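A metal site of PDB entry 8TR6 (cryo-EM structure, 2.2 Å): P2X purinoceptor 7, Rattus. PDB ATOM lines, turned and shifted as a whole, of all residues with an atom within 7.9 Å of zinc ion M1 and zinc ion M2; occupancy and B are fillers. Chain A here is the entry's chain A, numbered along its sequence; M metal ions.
N of Cys 572 lies close to SG of Cys 482, at 3.3 Å. N of Gly 480 lies close to SG of Cys 477 (3.2 Å). SG of Cys 506 sits close to OG1 of Thr 508, at 2.8 Å. N of Cys 498 lies within hydrogen-bond range of OE1 of Gln 422 (2.5 Å). The backbone NH (N) of Gly 504 lies within hydrogen-bond range of the backbone carbonyl oxygen (O) of Gln 478, 3.2 Å away. The backbone carbonyl oxygen (O) of Cys 499 lies within hydrogen-bond range of the backbone NH (N) of Val 404 (2.9 Å). SG of Cys 572 lies close to SG of Cys 573 (3.7 Å). The side-chain sulfur (SG) of Cys 498 sits close to the backbone NH (N) of Arg 500, at 3.7 Å.
Residues that only touch zinc ion M1: Gln 478 (3.8 Å). Along chain A the residues within 4 Å of zinc ion M1 span positions 477 to 498.
Within 4 Å of zinc ion M2: Cys 479, Cys 499, Cys 506 and Cys 572.
Zinc ion M1 is bound by SG of Cys 479 (2.3 Å), SG of Cys 482 (2.3 Å), SG of Cys 498 (2.3 Å) and SG of Cys 477 (2.3 Å).
SG of Cys 572 is bound to zinc ion M2, 2.3 Å away. Zinc ion M2 is bound by SG of Cys 479. Zinc ion M2 is bound by SG of Cys 506 (2.3 Å). Zinc ion M2 is bound by SG of Cys 499 (2.3 Å).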
ATOM      1  N   VAL A 404      -8.059 -32.350 -22.186  1.00  0.00           N
ATOM      2  CA  VAL A 404      -6.640 -32.185 -22.456  1.00  0.00           C
ATOM      3  C   VAL A 404      -5.979 -33.528 -22.709  1.00  0.00           C
ATOM      4  O   VAL A 404      -5.018 -33.627 -23.483  1.00  0.00           O
ATOM      5  CB  VAL A 404      -5.966 -31.426 -21.287  1.00  0.00           C
ATOM      6  CG1 VAL A 404      -5.664 -32.373 -20.136  1.00  0.00           C
ATOM      7  CG2 VAL A 404      -4.716 -30.725 -21.768  1.00  0.00           C
ATOM      8  N   GLN A 422     -19.714 -35.084 -18.025  1.00  0.00           N
ATOM      9  CA  GLN A 422     -18.482 -35.857 -18.126  1.00  0.00           C
ATOM     10  C   GLN A 422     -18.754 -37.293 -18.553  1.00  0.00           C
ATOM     11  O   GLN A 422     -18.008 -37.869 -19.344  1.00  0.00           O
ATOM     12  CB  GLN A 422     -17.749 -35.843 -16.774  1.00  0.00           C
ATOM     13  CG  GLN A 422     -16.334 -36.373 -16.844  1.00  0.00           C
ATOM     14  CD  GLN A 422     -15.301 -35.293 -17.086  1.00  0.00           C
ATOM     15  OE1 GLN A 422     -15.635 -34.119 -17.188  1.00  0.00           O
ATOM     16  NE2 GLN A 422     -14.036 -35.691 -17.171  1.00  0.00           N
ATOM     17  N   SER A 473     -12.909 -33.097  -3.875  1.00  0.00           N
ATOM     18  CA  SER A 473     -13.155 -32.940  -5.305  1.00  0.00           C
ATOM     19  C   SER A 473     -14.341 -33.798  -5.736  1.00  0.00           C
ATOM     20  O   SER A 473     -14.596 -34.858  -5.159  1.00  0.00           O
ATOM     21  CB  SER A 473     -11.908 -33.328  -6.095  1.00  0.00           C
ATOM     22  OG  SER A 473     -11.609 -34.700  -5.922  1.00  0.00           O
ATOM     23  N   PRO A 474     -15.083 -33.362  -6.756  1.00  0.00           N
ATOM     24  CA  PRO A 474     -16.204 -34.176  -7.238  1.00  0.00           C
ATOM     25  C   PRO A 474     -15.729 -35.515  -7.784  1.00  0.00           C
ATOM     26  O   PRO A 474     -14.602 -35.649  -8.261  1.00  0.00           O
ATOM     27  CB  PRO A 474     -16.826 -33.314  -8.346  1.00  0.00           C
ATOM     28  CG  PRO A 474     -16.357 -31.932  -8.085  1.00  0.00           C
ATOM     29  CD  PRO A 474     -15.008 -32.070  -7.456  1.00  0.00           C
ATOM     30  N   TRP A 476     -16.714 -37.127 -10.447  1.00  0.00           N
ATOM     31  CA  TRP A 476     -16.460 -37.065 -11.881  1.00  0.00           C
ATOM     32  C   TRP A 476     -15.174 -36.321 -12.214  1.00  0.00           C
ATOM     33  O   TRP A 476     -14.619 -36.506 -13.297  1.00  0.00           O
ATOM     34  CB  TRP A 476     -17.641 -36.414 -12.610  1.00  0.00           C
ATOM     35  CG  TRP A 476     -18.122 -35.146 -11.981  1.00  0.00           C
ATOM     36  CD1 TRP A 476     -19.201 -34.987 -11.159  1.00  0.00           C
ATOM     37  CD2 TRP A 476     -17.546 -33.839 -12.124  1.00  0.00           C
ATOM     38  NE1 TRP A 476     -19.332 -33.667 -10.785  1.00  0.00           N
ATOM     39  CE2 TRP A 476     -18.323 -32.944 -11.360  1.00  0.00           C
ATOM     40  CE3 TRP A 476     -16.440 -33.335 -12.822  1.00  0.00           C
ATOM     41  CZ2 TRP A 476     -18.036 -31.585 -11.282  1.00  0.00           C
ATOM     42  CZ3 TRP A 476     -16.152 -31.989 -12.738  1.00  0.00           C
ATOM     43  CH2 TRP A 476     -16.948 -31.126 -11.971  1.00  0.00           C
ATOM     44  N   CYS A 477     -14.690 -35.477 -11.302  1.00  0.00           N
ATOM     45  CA  CYS A 477     -13.472 -34.721 -11.552  1.00  0.00           C
ATOM     46  C   CYS A 477     -12.250 -35.636 -11.517  1.00  0.00           C
ATOM     47  O   CYS A 477     -12.233 -36.666 -10.842  1.00  0.00           O
ATOM     48  CB  CYS A 477     -13.308 -33.603 -10.529  1.00  0.00           C
ATOM     49  SG  CYS A 477     -11.717 -32.763 -10.611  1.00  0.00           S
ATOM     50  N   GLN A 478     -11.215 -35.235 -12.260  1.00  0.00           N
ATOM     51  CA  GLN A 478      -9.966 -35.973 -12.336  1.00  0.00           C
ATOM     52  C   GLN A 478      -8.759 -35.046 -12.273  1.00  0.00           C
ATOM     53  O   GLN A 478      -7.642 -35.463 -12.602  1.00  0.00           O
ATOM     54  CB  GLN A 478      -9.896 -36.816 -13.618  1.00  0.00           C
ATOM     55  CG  GLN A 478     -11.238 -37.395 -14.074  1.00  0.00           C
ATOM     56  CD  GLN A 478     -11.785 -38.434 -13.130  1.00  0.00           C
ATOM     57  OE1 GLN A 478     -11.026 -39.146 -12.463  1.00  0.00           O
ATOM     58  NE2 GLN A 478     -13.110 -38.542 -13.058  1.00  0.00           N
ATOM     59  N   CYS A 479      -8.953 -33.795 -11.852  1.00  0.00           N
ATOM     60  CA  CYS A 479      -7.878 -32.822 -11.778  1.00  0.00           C
ATOM     61  C   CYS A 479      -7.705 -32.219 -10.395  1.00  0.00           C
ATOM     62  O   CYS A 479      -6.663 -31.614 -10.126  1.00  0.00           O
ATOM     63  CB  CYS A 479      -8.085 -31.695 -12.802  1.00  0.00           C
ATOM     64  SG  CYS A 479      -9.323 -30.465 -12.332  1.00  0.00           S
ATOM     65  N   GLY A 480      -8.694 -32.351  -9.511  1.00  0.00           N
ATOM     66  CA  GLY A 480      -8.584 -31.860  -8.161  1.00  0.00           C
ATOM     67  C   GLY A 480      -8.900 -30.386  -7.982  1.00  0.00           C
ATOM     68  O   GLY A 480      -8.815 -29.894  -6.853  1.00  0.00           O
ATOM     69  N   ASN A 481      -9.261 -29.676  -9.050  1.00  0.00           N
ATOM     70  CA  ASN A 481      -9.581 -28.261  -8.967  1.00  0.00           C
ATOM     71  C   ASN A 481     -11.036 -27.951  -9.285  1.00  0.00           C
ATOM     72  O   ASN A 481     -11.468 -26.820  -9.062  1.00  0.00           O
ATOM     73  CB  ASN A 481      -8.678 -27.453  -9.919  1.00  0.00           C
ATOM     74  CG  ASN A 481      -7.223 -27.537  -9.542  1.00  0.00           C
ATOM     75  OD1 ASN A 481      -6.780 -28.498  -8.911  1.00  0.00           O
ATOM     76  ND2 ASN A 481      -6.450 -26.532  -9.928  1.00  0.00           N
ATOM     77  N   CYS A 482     -11.799 -28.921  -9.798  1.00  0.00           N
ATOM     78  CA  CYS A 482     -13.201 -28.693 -10.093  1.00  0.00           C
ATOM     79  C   CYS A 482     -14.014 -28.601  -8.803  1.00  0.00           C
ATOM     80  O   CYS A 482     -13.643 -29.171  -7.771  1.00  0.00           O
ATOM     81  CB  CYS A 482     -13.752 -29.808 -10.970  1.00  0.00           C
ATOM     82  SG  CYS A 482     -13.071 -29.847 -12.652  1.00  0.00           S
ATOM     83  N   LEU A 483     -15.116 -27.869  -8.871  1.00  0.00           N
ATOM     84  CA  LEU A 483     -16.008 -27.650  -7.745  1.00  0.00           C
ATOM     85  C   LEU A 483     -17.434 -27.937  -8.154  1.00  0.00           C
ATOM     86  O   LEU A 483     -17.777 -27.866  -9.341  1.00  0.00           O
ATOM     87  CB  LEU A 483     -15.895 -26.215  -7.232  1.00  0.00           C
ATOM     88  CG  LEU A 483     -14.473 -25.727  -6.919  1.00  0.00           C
ATOM     89  CD1 LEU A 483     -14.486 -24.240  -6.590  1.00  0.00           C
ATOM     90  CD2 LEU A 483     -13.877 -26.527  -5.775  1.00  0.00           C
ATOM     91  N   LEU A 497     -18.338 -30.983 -15.473  1.00  0.00           N
ATOM     92  CA  LEU A 497     -17.361 -31.335 -16.495  1.00  0.00           C
ATOM     93  C   LEU A 497     -15.967 -30.991 -16.000  1.00  0.00           C
ATOM     94  O   LEU A 497     -15.752 -29.936 -15.407  1.00  0.00           O
ATOM     95  CB  LEU A 497     -17.666 -30.599 -17.812  1.00  0.00           C
ATOM     96  CG  LEU A 497     -16.683 -30.772 -18.971  1.00  0.00           C
ATOM     97  CD1 LEU A 497     -16.837 -32.135 -19.625  1.00  0.00           C
ATOM     98  CD2 LEU A 497     -16.893 -29.663 -19.983  1.00  0.00           C
ATOM     99  N   CYS A 498     -15.020 -31.885 -16.258  1.00  0.00           N
ATOM    100  CA  CYS A 498     -13.627 -31.712 -15.878  1.00  0.00           C
ATOM    101  C   CYS A 498     -12.770 -31.498 -17.114  1.00  0.00           C
ATOM    102  O   CYS A 498     -13.156 -31.834 -18.234  1.00  0.00           O
ATOM    103  CB  CYS A 498     -13.122 -32.923 -15.082  1.00  0.00           C
ATOM    104  SG  CYS A 498     -11.441 -32.773 -14.463  1.00  0.00           S
ATOM    105  N   CYS A 499     -11.582 -30.931 -16.886  1.00  0.00           N
ATOM    106  CA  CYS A 499     -10.652 -30.630 -17.971  1.00  0.00           C
ATOM    107  C   CYS A 499     -10.017 -31.883 -18.574  1.00  0.00           C
ATOM    108  O   CYS A 499      -9.385 -31.766 -19.630  1.00  0.00           O
ATOM    109  CB  CYS A 499      -9.551 -29.705 -17.468  1.00  0.00           C
ATOM    110  SG  CYS A 499      -8.570 -30.360 -16.097  1.00  0.00           S
ATOM    111  N   ARG A 500     -10.167 -33.043 -17.943  1.00  0.00           N
ATOM    112  CA  ARG A 500      -9.536 -34.249 -18.436  1.00  0.00           C
ATOM    113  C   ARG A 500     -10.428 -35.441 -18.138  1.00  0.00           C
ATOM    114  O   ARG A 500     -11.296 -35.398 -17.262  1.00  0.00           O
ATOM    115  CB  ARG A 500      -8.144 -34.459 -17.811  1.00  0.00           C
ATOM    116  CG  ARG A 500      -8.104 -34.247 -16.304  1.00  0.00           C
ATOM    117  CD  ARG A 500      -6.693 -34.337 -15.755  1.00  0.00           C
ATOM    118  NE  ARG A 500      -5.833 -35.186 -16.572  1.00  0.00           N
ATOM    119  CZ  ARG A 500      -4.703 -34.789 -17.154  1.00  0.00           C
ATOM    120  NH1 ARG A 500      -4.252 -33.557 -17.033  1.00  0.00           N
ATOM    121  NH2 ARG A 500      -4.012 -35.660 -17.881  1.00  0.00           N
ATOM    122  N   GLY A 504      -4.844 -36.561 -13.554  1.00  0.00           N
ATOM    123  CA  GLY A 504      -3.623 -35.903 -13.973  1.00  0.00           C
ATOM    124  C   GLY A 504      -3.649 -34.435 -13.566  1.00  0.00           C
ATOM    125  O   GLY A 504      -4.513 -34.004 -12.812  1.00  0.00           O
ATOM    126  N   GLN A 505      -2.675 -33.705 -14.084  1.00  0.00           N
ATOM    127  CA  GLN A 505      -2.552 -32.288 -13.757  1.00  0.00           C
ATOM    128  C   GLN A 505      -3.639 -31.477 -14.435  1.00  0.00           C
ATOM    129  O   GLN A 505      -4.007 -31.736 -15.581  1.00  0.00           O
ATOM    130  CB  GLN A 505      -1.169 -31.766 -14.156  1.00  0.00           C
ATOM    131  CG  GLN A 505      -0.787 -32.037 -15.599  1.00  0.00           C
ATOM    132  CD  GLN A 505       0.414 -31.225 -16.047  1.00  0.00           C
ATOM    133  OE1 GLN A 505       0.671 -30.142 -15.520  1.00  0.00           O
ATOM    134  NE2 GLN A 505       1.160 -31.754 -17.004  1.00  0.00           N
ATOM    135  N   CYS A 506      -4.157 -30.483 -13.711  1.00  0.00           N
ATOM    136  CA  CYS A 506      -5.193 -29.625 -14.258  1.00  0.00           C
ATOM    137  C   CYS A 506      -4.624 -28.728 -15.352  1.00  0.00           C
ATOM    138  O   CYS A 506      -3.466 -28.287 -15.294  1.00  0.00           O
ATOM    139  CB  CYS A 506      -5.810 -28.769 -13.161  1.00  0.00           C
ATOM    140  SG  CYS A 506      -7.166 -27.711 -13.718  1.00  0.00           S
ATOM    141  N   ILE A 507      -5.447 -28.459 -16.362  1.00  0.00           N
ATOM    142  CA  ILE A 507      -5.028 -27.572 -17.445  1.00  0.00           C
ATOM    143  C   ILE A 507      -4.800 -26.161 -16.923  1.00  0.00           C
ATOM    144  O   ILE A 507      -4.005 -25.408 -17.493  1.00  0.00           O
ATOM    145  CB  ILE A 507      -6.085 -27.592 -18.574  1.00  0.00           C
ATOM    146  CG1 ILE A 507      -5.539 -26.863 -19.810  1.00  0.00           C
ATOM    147  CG2 ILE A 507      -7.373 -26.945 -18.103  1.00  0.00           C
ATOM    148  CD1 ILE A 507      -6.485 -26.871 -20.973  1.00  0.00           C
ATOM    149  N   THR A 508      -5.486 -25.792 -15.842  1.00  0.00           N
ATOM    150  CA  THR A 508      -5.305 -24.459 -15.283  1.00  0.00           C
ATOM    151  C   THR A 508      -3.879 -24.238 -14.784  1.00  0.00           C
ATOM    152  O   THR A 508      -3.404 -23.099 -14.739  1.00  0.00           O
ATOM    153  CB  THR A 508      -6.297 -24.220 -14.147  1.00  0.00           C
ATOM    154  OG1 THR A 508      -6.076 -25.179 -13.104  1.00  0.00           O
ATOM    155  CG2 THR A 508      -7.728 -24.326 -14.640  1.00  0.00           C
ATOM    156  N   THR A 509      -3.201 -25.318 -14.394  1.00  0.00           N
ATOM    157  CA  THR A 509      -1.841 -25.185 -13.880  1.00  0.00           C
ATOM    158  C   THR A 509      -0.865 -24.677 -14.936  1.00  0.00           C
ATOM    159  O   THR A 509       0.176 -24.126 -14.582  1.00  0.00           O
ATOM    160  CB  THR A 509      -1.351 -26.526 -13.335  1.00  0.00           C
ATOM    161  OG1 THR A 509      -1.407 -27.520 -14.373  1.00  0.00           O
ATOM    162  CG2 THR A 509      -2.221 -26.974 -12.174  1.00  0.00           C
ATOM    163  N   PHE A 513      -2.490 -21.044 -19.733  1.00  0.00           N
ATOM    164  CA  PHE A 513      -3.857 -20.804 -19.307  1.00  0.00           C
ATOM    165  C   PHE A 513      -3.994 -19.426 -18.684  1.00  0.00           C
ATOM    166  O   PHE A 513      -4.926 -18.670 -18.987  1.00  0.00           O
ATOM    167  CB  PHE A 513      -4.301 -21.888 -18.319  1.00  0.00           C
ATOM    168  CG  PHE A 513      -5.724 -21.745 -17.866  1.00  0.00           C
ATOM    169  CD1 PHE A 513      -6.050 -20.926 -16.800  1.00  0.00           C
ATOM    170  CD2 PHE A 513      -6.741 -22.439 -18.501  1.00  0.00           C
ATOM    171  CE1 PHE A 513      -7.358 -20.808 -16.381  1.00  0.00           C
ATOM    172  CE2 PHE A 513      -8.045 -22.315 -18.089  1.00  0.00           C
ATOM    173  CZ  PHE A 513      -8.353 -21.495 -17.024  1.00  0.00           C
ATOM    174  N   TYR A 553     -10.867 -19.067 -23.682  1.00  0.00           N
ATOM    175  CA  TYR A 553     -10.631 -20.486 -23.443  1.00  0.00           C
ATOM    176  C   TYR A 553     -11.326 -21.332 -24.509  1.00  0.00           C
ATOM    177  O   TYR A 553     -10.741 -22.288 -25.025  1.00  0.00           O
ATOM    178  CB  TYR A 553     -11.124 -20.888 -22.057  1.00  0.00           C
ATOM    179  CG  TYR A 553     -11.001 -22.372 -21.785  1.00  0.00           C
ATOM    180  CD1 TYR A 553     -11.999 -23.256 -22.172  1.00  0.00           C
ATOM    181  CD2 TYR A 553      -9.870 -22.897 -21.172  1.00  0.00           C
ATOM    182  CE1 TYR A 553     -11.876 -24.609 -21.936  1.00  0.00           C
ATOM    183  CE2 TYR A 553      -9.741 -24.247 -20.928  1.00  0.00           C
ATOM    184  CZ  TYR A 553     -10.754 -25.102 -21.316  1.00  0.00           C
ATOM    185  OH  TYR A 553     -10.633 -26.442 -21.084  1.00  0.00           O
ATOM    186  N   PRO A 570     -14.741 -26.458 -18.621  1.00  0.00           N
ATOM    187  CA  PRO A 570     -14.620 -27.313 -17.438  1.00  0.00           C
ATOM    188  C   PRO A 570     -14.907 -26.532 -16.173  1.00  0.00           C
ATOM    189  O   PRO A 570     -14.711 -25.317 -16.100  1.00  0.00           O
ATOM    190  CB  PRO A 570     -13.160 -27.799 -17.485  1.00  0.00           C
ATOM    191  CG  PRO A 570     -12.745 -27.619 -18.891  1.00  0.00           C
ATOM    192  CD  PRO A 570     -13.495 -26.443 -19.407  1.00  0.00           C
ATOM    193  N   SER A 571     -15.385 -27.250 -15.147  1.00  0.00           N
ATOM    194  CA  SER A 571     -15.718 -26.600 -13.892  1.00  0.00           C
ATOM    195  C   SER A 571     -14.496 -25.927 -13.274  1.00  0.00           C
ATOM    196  O   SER A 571     -14.582 -24.813 -12.753  1.00  0.00           O
ATOM    197  CB  SER A 571     -16.310 -27.619 -12.916  1.00  0.00           C
ATOM    198  OG  SER A 571     -16.528 -27.036 -11.644  1.00  0.00           O
ATOM    199  N   CYS A 572     -13.340 -26.590 -13.332  1.00  0.00           N
ATOM    200  CA  CYS A 572     -12.129 -26.023 -12.752  1.00  0.00           C
ATOM    201  C   CYS A 572     -11.772 -24.690 -13.411  1.00  0.00           C
ATOM    202  O   CYS A 572     -11.566 -23.681 -12.730  1.00  0.00           O
ATOM    203  CB  CYS A 572     -10.968 -27.006 -12.902  1.00  0.00           C
ATOM    204  SG  CYS A 572     -10.865 -27.773 -14.537  1.00  0.00           S
ATOM    205  N   CYS A 573     -11.693 -24.686 -14.745  1.00  0.00           N
ATOM    206  CA  CYS A 573     -11.343 -23.464 -15.458  1.00  0.00           C
ATOM    207  C   CYS A 573     -12.410 -22.385 -15.268  1.00  0.00           C
ATOM    208  O   CYS A 573     -12.089 -21.210 -15.059  1.00  0.00           O
ATOM    209  CB  CYS A 573     -11.148 -23.777 -16.941  1.00  0.00           C
ATOM    210  SG  CYS A 573     -10.223 -25.297 -17.245  1.00  0.00           S
HETATM  211 ZN    ZN M   1     -11.402 -31.470 -12.530  1.00  0.00          ZN
HETATM  212 ZN    ZN M   2      -8.985 -29.091 -14.182  1.00  0.00          ZN
